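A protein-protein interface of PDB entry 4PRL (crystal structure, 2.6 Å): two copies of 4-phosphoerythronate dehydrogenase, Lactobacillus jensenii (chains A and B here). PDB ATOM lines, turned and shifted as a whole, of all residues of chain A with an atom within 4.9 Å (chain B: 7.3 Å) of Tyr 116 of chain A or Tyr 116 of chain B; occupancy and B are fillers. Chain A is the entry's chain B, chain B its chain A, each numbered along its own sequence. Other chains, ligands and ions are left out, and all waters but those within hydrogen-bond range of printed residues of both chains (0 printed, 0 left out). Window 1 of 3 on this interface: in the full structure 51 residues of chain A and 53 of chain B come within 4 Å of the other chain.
Tyr 116 of chain A touches just these residues of chain B: Thr 112 (3.4 Å) and Tyr 116 (3.3 Å). Tyr 116 of chain B touches just these residues of chain A: Thr 112 and Tyr 116. Of the printed residues of chain B, Thr 112 of chain A touches Met 115 (3.2 Å), Tyr 116 (3.4 Å), Arg 119 (3.9 Å) and Ile 121 (3.9 Å). Of the printed residues of chain A, Arg 119 of chain B touches Thr 112. Lys 120 of chain A touches none of the printed residues of chain B. The nearest residue of chain B that does not touch Tyr 116 of chain A is Ile 291 of chain B (4.4 Å). The nearest residue of chain A that does not touch Tyr 116 of chain B is Ile 291 of chain A (4.2 Å).
The side-chain sulfur (SD) of Met 115 of chain B lies close to the side-chain hydroxyl (OG1) of Thr 112 of chain A.
Thr 112 of chain A touches Met 115 of chain B, and with the chains exchanged Met 115 of chain A touches Thr 112 of chain B. Thr 112 of chain A touches Tyr 116 of chain B, and with the chains exchanged Tyr 116 of chain A touches Thr 112 of chain B. Gln 113 of chain A touches Ile 121 of chain B, but with the chains exchanged Ile 121 of chain A does not touch Gln 113 of chain B (4.1 Å). Tyr 116 of chain B touches its own counterpart, Tyr 116 of chain A. 13 positions are printed for both chains. Of the 15 pairs that touch across the chains among the printed residues, 11 have their exchanged pair printed and touching as well.
The side-chain amide nitrogen of Gln 113 of chain B is in hydrogen-bond range of the side-chain hydroxyl of Thr 293 of chain B. The backbone NH (N) of Ile 121 of chain B is in hydrogen-bond range of the backbone carbonyl oxygen (O) of Tyr 116 of chain B, 3.2 Å away. The side-chain hydroxyl (OH) of Tyr 116 of chain B is in hydrogen-bond range of the backbone NH (N) of Gly 122 of chain B, at 3.1 Å. The backbone carbonyl oxygen (O) of Tyr 116 of chain A sits at hydrogen-bond distance from the backbone NH (N) of Ile 121 of chain A (3.4 Å). The backbone NH (N) of Gly 122 of chain A lies close to the side-chain hydroxyl (OH) of Tyr 116 of chain A, 3.1 Å away.
Of the 25 printed residues of chain B, 8 touch a printed residue of chain A. Hydrophobic or aromatic side chains of chain B that line the printed part of chain A: Met 109, Met 115, Tyr 116, Ile 121 and Ile 291. Hydrophobic or aromatic side chains of chain A that line the printed part of chain B: Met 115, Tyr 116, Ile 121 and Ile 291. Among the printed residues, no Asp or Glu carboxylate lies within 4 Å of a Lys or Arg side-chain nitrogen of the other chain.
Among the printed residues, pairs that only touch across the chains: Thr 112 of chain A with Tyr 116 of chain B (3.4 Å), Thr 112 of chain A with Arg 119 of chain B (3.9 Å), Thr 112 of chain A with Ile 121 of chain B (3.9 Å), Gln 113 of chain A with Ile 121 of chain B (3.99 Å), Met 115 of chain A with Thr 112 of chain B (3.3 Å), Tyr 116 of chain A with Thr 112 of chain B (3.4 Å), Tyr 116 of chain A with Tyr 116 of chain B (3.3 Å), Arg 119 of chain A with Met 109 of chain B (3.8 Å), Arg 119 of chain A with Thr 112 of chain B (3.9 Å), Ile 121 of chain A with Met 109 of chain B (3.9 Å), Ile 121 of chain A with Thr 112 of chain B (3.9 Å), Ile 121 of chain A with Ile 291 of chain B (3.9 Å), Ile 121 of chain A with Thr 293 of chain B (3.7 Å) and Ile 291 of chain A with Ile 121 of chain B (3.9996 Å).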
ATOM      1  N   THR A 112      23.271   5.465 -20.937  1.00  0.00           N
ATOM      2  CA  THR A 112      23.477   6.577 -20.036  1.00  0.00           C
ATOM      3  C   THR A 112      24.744   7.367 -20.407  1.00  0.00           C
ATOM      4  O   THR A 112      24.721   8.616 -20.513  1.00  0.00           O
ATOM      5  CB  THR A 112      23.505   6.076 -18.581  1.00  0.00           C
ATOM      6  OG1 THR A 112      22.192   5.604 -18.238  1.00  0.00           O
ATOM      7  CG2 THR A 112      23.934   7.177 -17.623  1.00  0.00           C
ATOM      8  N   GLN A 113      25.839   6.648 -20.624  1.00  0.00           N
ATOM      9  CA  GLN A 113      27.082   7.316 -20.943  1.00  0.00           C
ATOM     10  C   GLN A 113      26.934   8.052 -22.249  1.00  0.00           C
ATOM     11  O   GLN A 113      27.351   9.206 -22.387  1.00  0.00           O
ATOM     12  CB  GLN A 113      28.220   6.314 -21.007  1.00  0.00           C
ATOM     13  CG  GLN A 113      28.609   5.847 -19.620  1.00  0.00           C
ATOM     14  CD  GLN A 113      29.949   5.172 -19.589  1.00  0.00           C
ATOM     15  OE1 GLN A 113      30.882   5.627 -20.222  1.00  0.00           O
ATOM     16  NE2 GLN A 113      30.059   4.097 -18.825  1.00  0.00           N
ATOM     17  N   ALA A 114      26.308   7.392 -23.199  1.00  0.00           N
ATOM     18  CA  ALA A 114      26.066   8.002 -24.485  1.00  0.00           C
ATOM     19  C   ALA A 114      25.263   9.327 -24.406  1.00  0.00           C
ATOM     20  O   ALA A 114      25.650  10.353 -24.990  1.00  0.00           O
ATOM     21  CB  ALA A 114      25.353   7.000 -25.360  1.00  0.00           C
ATOM     22  N   MET A 115      24.171   9.295 -23.658  1.00  0.00           N
ATOM     23  CA  MET A 115      23.357  10.477 -23.444  1.00  0.00           C
ATOM     24  C   MET A 115      24.206  11.626 -22.897  1.00  0.00           C
ATOM     25  O   MET A 115      24.239  12.725 -23.459  1.00  0.00           O
ATOM     26  CB  MET A 115      22.244  10.181 -22.447  1.00  0.00           C
ATOM     27  CG  MET A 115      21.409   8.943 -22.754  1.00  0.00           C
ATOM     28  SD  MET A 115      19.740   9.299 -23.306  1.00  0.00           S
ATOM     29  CE  MET A 115      20.143  10.065 -24.884  1.00  0.00           C
ATOM     30  N   TYR A 116      24.901  11.372 -21.794  1.00  0.00           N
ATOM     31  CA  TYR A 116      25.662  12.427 -21.121  1.00  0.00           C
ATOM     32  C   TYR A 116      26.679  13.113 -22.035  1.00  0.00           C
ATOM     33  O   TYR A 116      26.830  14.346 -22.032  1.00  0.00           O
ATOM     34  CB  TYR A 116      26.367  11.825 -19.929  1.00  0.00           C
ATOM     35  CG  TYR A 116      27.291  12.754 -19.204  1.00  0.00           C
ATOM     36  CD1 TYR A 116      28.584  12.972 -19.673  1.00  0.00           C
ATOM     37  CD2 TYR A 116      26.900  13.376 -18.021  1.00  0.00           C
ATOM     38  CE1 TYR A 116      29.451  13.804 -18.997  1.00  0.00           C
ATOM     39  CE2 TYR A 116      27.768  14.208 -17.337  1.00  0.00           C
ATOM     40  CZ  TYR A 116      29.039  14.415 -17.837  1.00  0.00           C
ATOM     41  OH  TYR A 116      29.920  15.231 -17.203  1.00  0.00           O
ATOM     42  N   LEU A 117      27.381  12.307 -22.819  1.00  0.00           N
ATOM     43  CA  LEU A 117      28.397  12.844 -23.724  1.00  0.00           C
ATOM     44  C   LEU A 117      27.747  13.602 -24.885  1.00  0.00           C
ATOM     45  O   LEU A 117      28.222  14.671 -25.306  1.00  0.00           O
ATOM     46  CB  LEU A 117      29.290  11.703 -24.206  1.00  0.00           C
ATOM     47  CG  LEU A 117      30.104  11.123 -23.035  1.00  0.00           C
ATOM     48  CD1 LEU A 117      30.741   9.777 -23.348  1.00  0.00           C
ATOM     49  CD2 LEU A 117      31.167  12.112 -22.584  1.00  0.00           C
ATOM     50  N   ASN A 118      26.627  13.069 -25.367  1.00  0.00           N
ATOM     51  CA  ASN A 118      25.885  13.761 -26.394  1.00  0.00           C
ATOM     52  C   ASN A 118      25.448  15.155 -25.936  1.00  0.00           C
ATOM     53  O   ASN A 118      25.461  16.093 -26.717  1.00  0.00           O
ATOM     54  CB  ASN A 118      24.655  12.956 -26.815  1.00  0.00           C
ATOM     55  CG  ASN A 118      23.910  13.615 -27.956  1.00  0.00           C
ATOM     56  OD1 ASN A 118      24.512  13.943 -28.973  1.00  0.00           O
ATOM     57  ND2 ASN A 118      22.625  13.861 -27.773  1.00  0.00           N
ATOM     58  N   ARG A 119      25.042  15.272 -24.676  1.00  0.00           N
ATOM     59  CA  ARG A 119      24.605  16.529 -24.148  1.00  0.00           C
ATOM     60  C   ARG A 119      25.768  17.378 -23.695  1.00  0.00           C
ATOM     61  O   ARG A 119      25.577  18.527 -23.327  1.00  0.00           O
ATOM     62  CB  ARG A 119      23.679  16.286 -22.986  1.00  0.00           C
ATOM     63  CG  ARG A 119      22.401  15.541 -23.346  1.00  0.00           C
ATOM     64  CD  ARG A 119      21.626  16.171 -24.485  1.00  0.00           C
ATOM     65  NE  ARG A 119      21.309  17.569 -24.222  1.00  0.00           N
ATOM     66  CZ  ARG A 119      20.118  18.131 -24.396  1.00  0.00           C
ATOM     67  NH1 ARG A 119      19.098  17.437 -24.857  1.00  0.00           N
ATOM     68  NH2 ARG A 119      19.954  19.418 -24.106  1.00  0.00           N
ATOM     69  N   LYS A 120      26.960  16.786 -23.673  1.00  0.00           N
ATOM     70  CA  LYS A 120      28.225  17.496 -23.437  1.00  0.00           C
ATOM     71  C   LYS A 120      28.361  18.107 -22.056  1.00  0.00           C
ATOM     72  O   LYS A 120      29.040  19.104 -21.833  1.00  0.00           O
ATOM     73  CB  LYS A 120      28.475  18.520 -24.532  1.00  0.00           C
ATOM     74  CG  LYS A 120      28.718  17.859 -25.875  1.00  0.00           C
ATOM     75  CD  LYS A 120      28.857  18.907 -26.963  1.00  0.00           C
ATOM     76  CE  LYS A 120      28.842  18.299 -28.345  1.00  0.00           C
ATOM     77  NZ  LYS A 120      28.519  19.384 -29.304  1.00  0.00           N
ATOM     78  N   ILE A 121      27.746  17.452 -21.106  1.00  0.00           N
ATOM     79  CA  ILE A 121      27.660  17.983 -19.766  1.00  0.00           C
ATOM     80  C   ILE A 121      29.039  18.153 -19.130  1.00  0.00           C
ATOM     81  O   ILE A 121      29.248  19.066 -18.349  1.00  0.00           O
ATOM     82  CB  ILE A 121      26.730  17.076 -18.944  1.00  0.00           C
ATOM     83  CG1 ILE A 121      25.273  17.277 -19.418  1.00  0.00           C
ATOM     84  CG2 ILE A 121      26.850  17.351 -17.464  1.00  0.00           C
ATOM     85  CD1 ILE A 121      24.360  16.113 -19.096  1.00  0.00           C
ATOM     86  N   GLY A 122      29.983  17.295 -19.490  1.00  0.00           N
ATOM     87  CA  GLY A 122      31.316  17.352 -18.919  1.00  0.00           C
ATOM     88  C   GLY A 122      32.131  18.498 -19.472  1.00  0.00           C
ATOM     89  O   GLY A 122      32.936  19.126 -18.753  1.00  0.00           O
ATOM     90  N   PRO A 288      37.264  16.197 -20.492  1.00  0.00           N
ATOM     91  CA  PRO A 288      35.851  16.414 -20.180  1.00  0.00           C
ATOM     92  C   PRO A 288      34.842  15.682 -21.078  1.00  0.00           C
ATOM     93  O   PRO A 288      33.722  15.434 -20.645  1.00  0.00           O
ATOM     94  CB  PRO A 288      35.687  17.923 -20.355  1.00  0.00           C
ATOM     95  CG  PRO A 288      36.682  18.288 -21.385  1.00  0.00           C
ATOM     96  CD  PRO A 288      37.846  17.359 -21.180  1.00  0.00           C
ATOM     97  N   ILE A 291      34.095   9.594 -20.392  1.00  0.00           N
ATOM     98  CA  ILE A 291      33.706   8.927 -19.163  1.00  0.00           C
ATOM     99  C   ILE A 291      34.485   7.614 -19.063  1.00  0.00           C
ATOM    100  O   ILE A 291      34.599   6.881 -20.045  1.00  0.00           O
ATOM    101  CB  ILE A 291      32.202   8.611 -19.170  1.00  0.00           C
ATOM    102  CG1 ILE A 291      31.368   9.876 -18.927  1.00  0.00           C
ATOM    103  CG2 ILE A 291      31.893   7.563 -18.123  1.00  0.00           C
ATOM    104  CD1 ILE A 291      29.877   9.695 -19.131  1.00  0.00           C
ATOM    105  N   MET B 109      17.495  16.257 -21.649  1.00  0.00           N
ATOM    106  CA  MET B 109      18.461  16.709 -20.641  1.00  0.00           C
ATOM    107  C   MET B 109      18.054  16.120 -19.267  1.00  0.00           C
ATOM    108  O   MET B 109      18.871  15.518 -18.571  1.00  0.00           O
ATOM    109  CB  MET B 109      18.563  18.241 -20.590  1.00  0.00           C
ATOM    110  CG  MET B 109      19.652  18.761 -19.661  1.00  0.00           C
ATOM    111  SD  MET B 109      21.324  18.250 -20.165  1.00  0.00           S
ATOM    112  CE  MET B 109      22.162  19.824 -20.118  1.00  0.00           C
ATOM    113  N   ALA B 110      16.779  16.238 -18.917  1.00  0.00           N
ATOM    114  CA  ALA B 110      16.328  15.801 -17.637  1.00  0.00           C
ATOM    115  C   ALA B 110      16.538  14.296 -17.514  1.00  0.00           C
ATOM    116  O   ALA B 110      17.092  13.843 -16.526  1.00  0.00           O
ATOM    117  CB  ALA B 110      14.873  16.187 -17.419  1.00  0.00           C
ATOM    118  N   VAL B 111      16.149  13.514 -18.522  1.00  0.00           N
ATOM    119  CA  VAL B 111      16.410  12.054 -18.476  1.00  0.00           C
ATOM    120  C   VAL B 111      17.910  11.746 -18.362  1.00  0.00           C
ATOM    121  O   VAL B 111      18.312  10.969 -17.503  1.00  0.00           O
ATOM    122  CB  VAL B 111      15.839  11.297 -19.679  1.00  0.00           C
ATOM    123  CG1 VAL B 111      16.301   9.835 -19.690  1.00  0.00           C
ATOM    124  CG2 VAL B 111      14.326  11.351 -19.641  1.00  0.00           C
ATOM    125  N   THR B 112      18.713  12.378 -19.213  1.00  0.00           N
ATOM    126  CA  THR B 112      20.157  12.173 -19.255  1.00  0.00           C
ATOM    127  C   THR B 112      20.798  12.377 -17.891  1.00  0.00           C
ATOM    128  O   THR B 112      21.502  11.489 -17.401  1.00  0.00           O
ATOM    129  CB  THR B 112      20.806  13.130 -20.273  1.00  0.00           C
ATOM    130  OG1 THR B 112      20.357  12.781 -21.571  1.00  0.00           O
ATOM    131  CG2 THR B 112      22.296  12.989 -20.282  1.00  0.00           C
ATOM    132  N   GLN B 113      20.545  13.531 -17.267  1.00  0.00           N
ATOM    133  CA  GLN B 113      21.081  13.807 -15.924  1.00  0.00           C
ATOM    134  C   GLN B 113      20.573  12.782 -14.873  1.00  0.00           C
ATOM    135  O   GLN B 113      21.352  12.297 -14.042  1.00  0.00           O
ATOM    136  CB  GLN B 113      20.729  15.222 -15.475  1.00  0.00           C
ATOM    137  CG  GLN B 113      21.342  16.344 -16.308  1.00  0.00           C
ATOM    138  CD  GLN B 113      21.269  17.704 -15.609  1.00  0.00           C
ATOM    139  OE1 GLN B 113      21.015  17.768 -14.425  1.00  0.00           O
ATOM    140  NE2 GLN B 113      21.519  18.788 -16.343  1.00  0.00           N
ATOM    141  N   ALA B 114      19.294  12.425 -14.917  1.00  0.00           N
ATOM    142  CA  ALA B 114      18.783  11.370 -14.026  1.00  0.00           C
ATOM    143  C   ALA B 114      19.517  10.016 -14.153  1.00  0.00           C
ATOM    144  O   ALA B 114      19.860   9.371 -13.163  1.00  0.00           O
ATOM    145  CB  ALA B 114      17.290  11.180 -14.224  1.00  0.00           C
ATOM    146  N   MET B 115      19.807   9.598 -15.365  1.00  0.00           N
ATOM    147  CA  MET B 115      20.456   8.326 -15.545  1.00  0.00           C
ATOM    148  C   MET B 115      21.899   8.365 -15.089  1.00  0.00           C
ATOM    149  O   MET B 115      22.389   7.438 -14.459  1.00  0.00           O
ATOM    150  CB  MET B 115      20.400   7.917 -16.996  1.00  0.00           C
ATOM    151  CG  MET B 115      19.038   8.131 -17.620  1.00  0.00           C
ATOM    152  SD  MET B 115      18.651   6.852 -18.794  1.00  0.00           S
ATOM    153  CE  MET B 115      18.647   5.488 -17.622  1.00  0.00           C
ATOM    154  N   TYR B 116      22.595   9.440 -15.416  1.00  0.00           N
ATOM    155  CA  TYR B 116      23.988   9.589 -14.983  1.00  0.00           C
ATOM    156  C   TYR B 116      24.105   9.518 -13.471  1.00  0.00           C
ATOM    157  O   TYR B 116      24.959   8.802 -12.938  1.00  0.00           O
ATOM    158  CB  TYR B 116      24.539  10.907 -15.475  1.00  0.00           C
ATOM    159  CG  TYR B 116      25.944  11.175 -15.049  1.00  0.00           C
ATOM    160  CD1 TYR B 116      26.195  11.783 -13.849  1.00  0.00           C
ATOM    161  CD2 TYR B 116      27.030  10.850 -15.874  1.00  0.00           C
ATOM    162  CE1 TYR B 116      27.481  12.043 -13.446  1.00  0.00           C
ATOM    163  CE2 TYR B 116      28.324  11.135 -15.488  1.00  0.00           C
ATOM    164  CZ  TYR B 116      28.537  11.718 -14.265  1.00  0.00           C
ATOM    165  OH  TYR B 116      29.785  12.016 -13.811  1.00  0.00           O
ATOM    166  N   LEU B 117      23.238  10.254 -12.779  1.00  0.00           N
ATOM    167  CA  LEU B 117      23.311  10.317 -11.327  1.00  0.00           C
ATOM    168  C   LEU B 117      22.854   9.009 -10.695  1.00  0.00           C
ATOM    169  O   LEU B 117      23.430   8.600  -9.667  1.00  0.00           O
ATOM    170  CB  LEU B 117      22.510  11.505 -10.782  1.00  0.00           C
ATOM    171  CG  LEU B 117      23.038  12.885 -11.200  1.00  0.00           C
ATOM    172  CD1 LEU B 117      22.042  13.962 -10.806  1.00  0.00           C
ATOM    173  CD2 LEU B 117      24.414  13.154 -10.614  1.00  0.00           C
ATOM    174  N   ASN B 118      21.853   8.357 -11.311  1.00  0.00           N
ATOM    175  CA  ASN B 118      21.425   6.999 -10.916  1.00  0.00           C
ATOM    176  C   ASN B 118      22.534   6.004 -11.059  1.00  0.00           C
ATOM    177  O   ASN B 118      22.707   5.182 -10.202  1.00  0.00           O
ATOM    178  CB  ASN B 118      20.254   6.478 -11.760  1.00  0.00           C
ATOM    179  CG  ASN B 118      19.807   5.062 -11.350  1.00  0.00           C
ATOM    180  OD1 ASN B 118      19.690   4.753 -10.173  1.00  0.00           O
ATOM    181  ND2 ASN B 118      19.547   4.216 -12.322  1.00  0.00           N
ATOM    182  N   ARG B 119      23.272   6.059 -12.158  1.00  0.00           N
ATOM    183  CA  ARG B 119      24.416   5.188 -12.323  1.00  0.00           C
ATOM    184  C   ARG B 119      25.590   5.666 -11.437  1.00  0.00           C
ATOM    185  O   ARG B 119      26.620   4.975 -11.330  1.00  0.00           O
ATOM    186  CB  ARG B 119      24.828   5.096 -13.789  1.00  0.00           C
ATOM    187  CG  ARG B 119      23.750   4.555 -14.713  1.00  0.00           C
ATOM    188  CD  ARG B 119      23.103   3.233 -14.286  1.00  0.00           C
ATOM    189  NE  ARG B 119      24.094   2.191 -13.961  1.00  0.00           N
ATOM    190  CZ  ARG B 119      24.129   0.944 -14.444  1.00  0.00           C
ATOM    191  NH1 ARG B 119      23.206   0.473 -15.264  1.00  0.00           N
ATOM    192  NH2 ARG B 119      25.098   0.137 -14.054  1.00  0.00           N
ATOM    193  N   LYS B 120      25.437   6.844 -10.821  1.00  0.00           N
ATOM    194  CA  LYS B 120      26.412   7.376  -9.889  1.00  0.00           C
ATOM    195  C   LYS B 120      27.787   7.503 -10.513  1.00  0.00           C
ATOM    196  O   LYS B 120      28.801   7.284  -9.859  1.00  0.00           O
ATOM    197  CB  LYS B 120      26.491   6.492  -8.653  1.00  0.00           C
ATOM    198  CG  LYS B 120      25.179   6.392  -7.906  1.00  0.00           C
ATOM    199  CD  LYS B 120      25.276   5.421  -6.748  1.00  0.00           C
ATOM    200  CE  LYS B 120      23.995   5.433  -5.946  1.00  0.00           C
ATOM    201  NZ  LYS B 120      23.837   4.157  -5.216  1.00  0.00           N
ATOM    202  N   ILE B 121      27.813   7.870 -11.780  1.00  0.00           N
ATOM    203  CA  ILE B 121      29.060   7.920 -12.530  1.00  0.00           C
ATOM    204  C   ILE B 121      30.070   8.920 -11.956  1.00  0.00           C
ATOM    205  O   ILE B 121      31.274   8.665 -11.990  1.00  0.00           O
ATOM    206  CB  ILE B 121      28.789   8.206 -14.026  1.00  0.00           C
ATOM    207  CG1 ILE B 121      28.212   6.938 -14.689  1.00  0.00           C
ATOM    208  CG2 ILE B 121      30.049   8.652 -14.745  1.00  0.00           C
ATOM    209  CD1 ILE B 121      27.510   7.177 -16.024  1.00  0.00           C
ATOM    210  N   GLY B 122      29.588  10.041 -11.428  1.00  0.00           N
ATOM    211  CA  GLY B 122      30.454  11.054 -10.839  1.00  0.00           C
ATOM    212  C   GLY B 122      31.002  10.663  -9.481  1.00  0.00           C
ATOM    213  O   GLY B 122      32.090  11.091  -9.109  1.00  0.00           O
ATOM    214  N   GLU B 123      30.254   9.851  -8.736  1.00  0.00           N
ATOM    215  CA  GLU B 123      30.732   9.353  -7.451  1.00  0.00           C
ATOM    216  C   GLU B 123      31.815   8.312  -7.703  1.00  0.00           C
ATOM    217  O   GLU B 123      32.841   8.302  -7.021  1.00  0.00           O
ATOM    218  CB  GLU B 123      29.593   8.783  -6.606  1.00  0.00           C
ATOM    219  CG  GLU B 123      28.493   9.786  -6.258  1.00  0.00           C
ATOM    220  CD  GLU B 123      27.317   9.134  -5.533  1.00  0.00           C
ATOM    221  OE1 GLU B 123      27.516   8.696  -4.387  1.00  0.00           O
ATOM    222  OE2 GLU B 123      26.194   9.048  -6.091  1.00  0.00           O
ATOM    223  N   PHE B 124      31.613   7.455  -8.699  1.00  0.00           N
ATOM    224  CA  PHE B 124      32.697   6.585  -9.160  1.00  0.00           C
ATOM    225  C   PHE B 124      33.929   7.365  -9.562  1.00  0.00           C
ATOM    226  O   PHE B 124      35.036   6.940  -9.263  1.00  0.00           O
ATOM    227  CB  PHE B 124      32.307   5.774 -10.384  1.00  0.00           C
ATOM    228  CG  PHE B 124      31.538   4.532 -10.076  1.00  0.00           C
ATOM    229  CD1 PHE B 124      32.177   3.435  -9.537  1.00  0.00           C
ATOM    230  CD2 PHE B 124      30.180   4.452 -10.373  1.00  0.00           C
ATOM    231  CE1 PHE B 124      31.487   2.290  -9.264  1.00  0.00           C
ATOM    232  CE2 PHE B 124      29.491   3.316 -10.098  1.00  0.00           C
ATOM    233  CZ  PHE B 124      30.144   2.229  -9.548  1.00  0.00           C
ATOM    234  N   LYS B 125      33.756   8.464 -10.291  1.00  0.00           N
ATOM    235  CA  LYS B 125      34.919   9.226 -10.735  1.00  0.00           C
ATOM    236  C   LYS B 125      35.637   9.837  -9.534  1.00  0.00           C
ATOM    237  O   LYS B 125      36.873   9.823  -9.470  1.00  0.00           O
ATOM    238  CB  LYS B 125      34.543  10.328 -11.730  1.00  0.00           C
ATOM    239  CG  LYS B 125      35.735  10.900 -12.507  1.00  0.00           C
ATOM    240  CD  LYS B 125      35.391  12.215 -13.215  1.00  0.00           C
ATOM    241  CE  LYS B 125      36.060  12.342 -14.583  1.00  0.00           C
ATOM    242  NZ  LYS B 125      37.545  12.329 -14.467  1.00  0.00           N
ATOM    243  N   SER B 141      23.782   0.426  -8.263  1.00  0.00           N
ATOM    244  CA  SER B 141      22.721   1.145  -8.966  1.00  0.00           C
ATOM    245  C   SER B 141      21.512   0.246  -9.157  1.00  0.00           C
ATOM    246  O   SER B 141      21.324  -0.745  -8.438  1.00  0.00           O
ATOM    247  CB  SER B 141      23.225   1.691 -10.312  1.00  0.00           C
ATOM    248  OG  SER B 141      22.320   2.642 -10.857  1.00  0.00           O
ATOM    249  N   ILE B 229      16.583  11.128  -6.318  1.00  0.00           N
ATOM    250  CA  ILE B 229      17.312  12.024  -7.217  1.00  0.00           C
ATOM    251  C   ILE B 229      16.340  13.125  -7.619  1.00  0.00           C
ATOM    252  O   ILE B 229      15.238  12.838  -8.071  1.00  0.00           O
ATOM    253  CB  ILE B 229      17.807  11.287  -8.477  1.00  0.00           C
ATOM    254  CG1 ILE B 229      18.647  10.070  -8.077  1.00  0.00           C
ATOM    255  CG2 ILE B 229      18.602  12.229  -9.380  1.00  0.00           C
ATOM    256  CD1 ILE B 229      19.036   9.163  -9.224  1.00  0.00           C
ATOM    257  N   ALA B 255      21.034  12.577  -4.942  1.00  0.00           N
ATOM    258  CA  ALA B 255      21.683  13.334  -6.004  1.00  0.00           C
ATOM    259  C   ALA B 255      20.757  14.406  -6.546  1.00  0.00           C
ATOM    260  O   ALA B 255      19.540  14.357  -6.340  1.00  0.00           O
ATOM    261  CB  ALA B 255      22.092  12.400  -7.131  1.00  0.00           C
ATOM    262  N   PRO B 288      30.200  15.225  -6.266  1.00  0.00           N
ATOM    263  CA  PRO B 288      30.208  14.278  -7.387  1.00  0.00           C
ATOM    264  C   PRO B 288      28.852  13.609  -7.664  1.00  0.00           C
ATOM    265  O   PRO B 288      28.673  13.006  -8.738  1.00  0.00           O
ATOM    266  CB  PRO B 288      31.221  13.233  -6.947  1.00  0.00           C
ATOM    267  CG  PRO B 288      31.123  13.231  -5.449  1.00  0.00           C
ATOM    268  CD  PRO B 288      30.774  14.637  -5.039  1.00  0.00           C
ATOM    269  N   ASN B 289      27.922  13.702  -6.711  1.00  0.00           N
ATOM    270  CA  ASN B 289      26.509  13.361  -6.950  1.00  0.00           C
ATOM    271  C   ASN B 289      25.638  14.558  -7.385  1.00  0.00           C
ATOM    272  O   ASN B 289      24.415  14.522  -7.263  1.00  0.00           O
ATOM    273  CB  ASN B 289      25.887  12.641  -5.723  1.00  0.00           C
ATOM    274  CG  ASN B 289      25.823  13.521  -4.459  1.00  0.00           C
ATOM    275  OD1 ASN B 289      26.603  14.450  -4.279  1.00  0.00           O
ATOM    276  ND2 ASN B 289      24.893  13.204  -3.575  1.00  0.00           N
ATOM    277  N   VAL B 290      26.256  15.607  -7.914  1.00  0.00           N
ATOM    278  CA  VAL B 290      25.501  16.729  -8.477  1.00  0.00           C
ATOM    279  C   VAL B 290      25.934  17.033  -9.911  1.00  0.00           C
ATOM    280  O   VAL B 290      27.110  16.850 -10.274  1.00  0.00           O
ATOM    281  CB  VAL B 290      25.721  17.996  -7.642  1.00  0.00           C
ATOM    282  CG1 VAL B 290      25.125  19.218  -8.323  1.00  0.00           C
ATOM    283  CG2 VAL B 290      25.138  17.804  -6.246  1.00  0.00           C
ATOM    284  N   ILE B 291      24.976  17.501 -10.714  1.00  0.00           N
ATOM    285  CA  ILE B 291      25.229  18.034 -12.042  1.00  0.00           C
ATOM    286  C   ILE B 291      24.663  19.450 -12.144  1.00  0.00           C
ATOM    287  O   ILE B 291      23.482  19.681 -11.887  1.00  0.00           O
ATOM    288  CB  ILE B 291      24.532  17.178 -13.107  1.00  0.00           C
ATOM    289  CG1 ILE B 291      25.267  15.858 -13.308  1.00  0.00           C
ATOM    290  CG2 ILE B 291      24.458  17.925 -14.432  1.00  0.00           C
ATOM    291  CD1 ILE B 291      24.612  14.946 -14.329  1.00  0.00           C
ATOM    292  N   THR B 293      24.306  22.200 -15.171  1.00  0.00           N
ATOM    293  CA  THR B 293      24.469  22.714 -16.511  1.00  0.00           C
ATOM    294  C   THR B 293      23.910  24.149 -16.541  1.00  0.00           C
ATOM    295  O   THR B 293      23.000  24.494 -15.767  1.00  0.00           O
ATOM    296  CB  THR B 293      23.711  21.831 -17.524  1.00  0.00           C
ATOM    297  OG1 THR B 293      22.409  21.491 -17.015  1.00  0.00           O
ATOM    298  CG2 THR B 293      24.474  20.549 -17.795  1.00  0.00           C
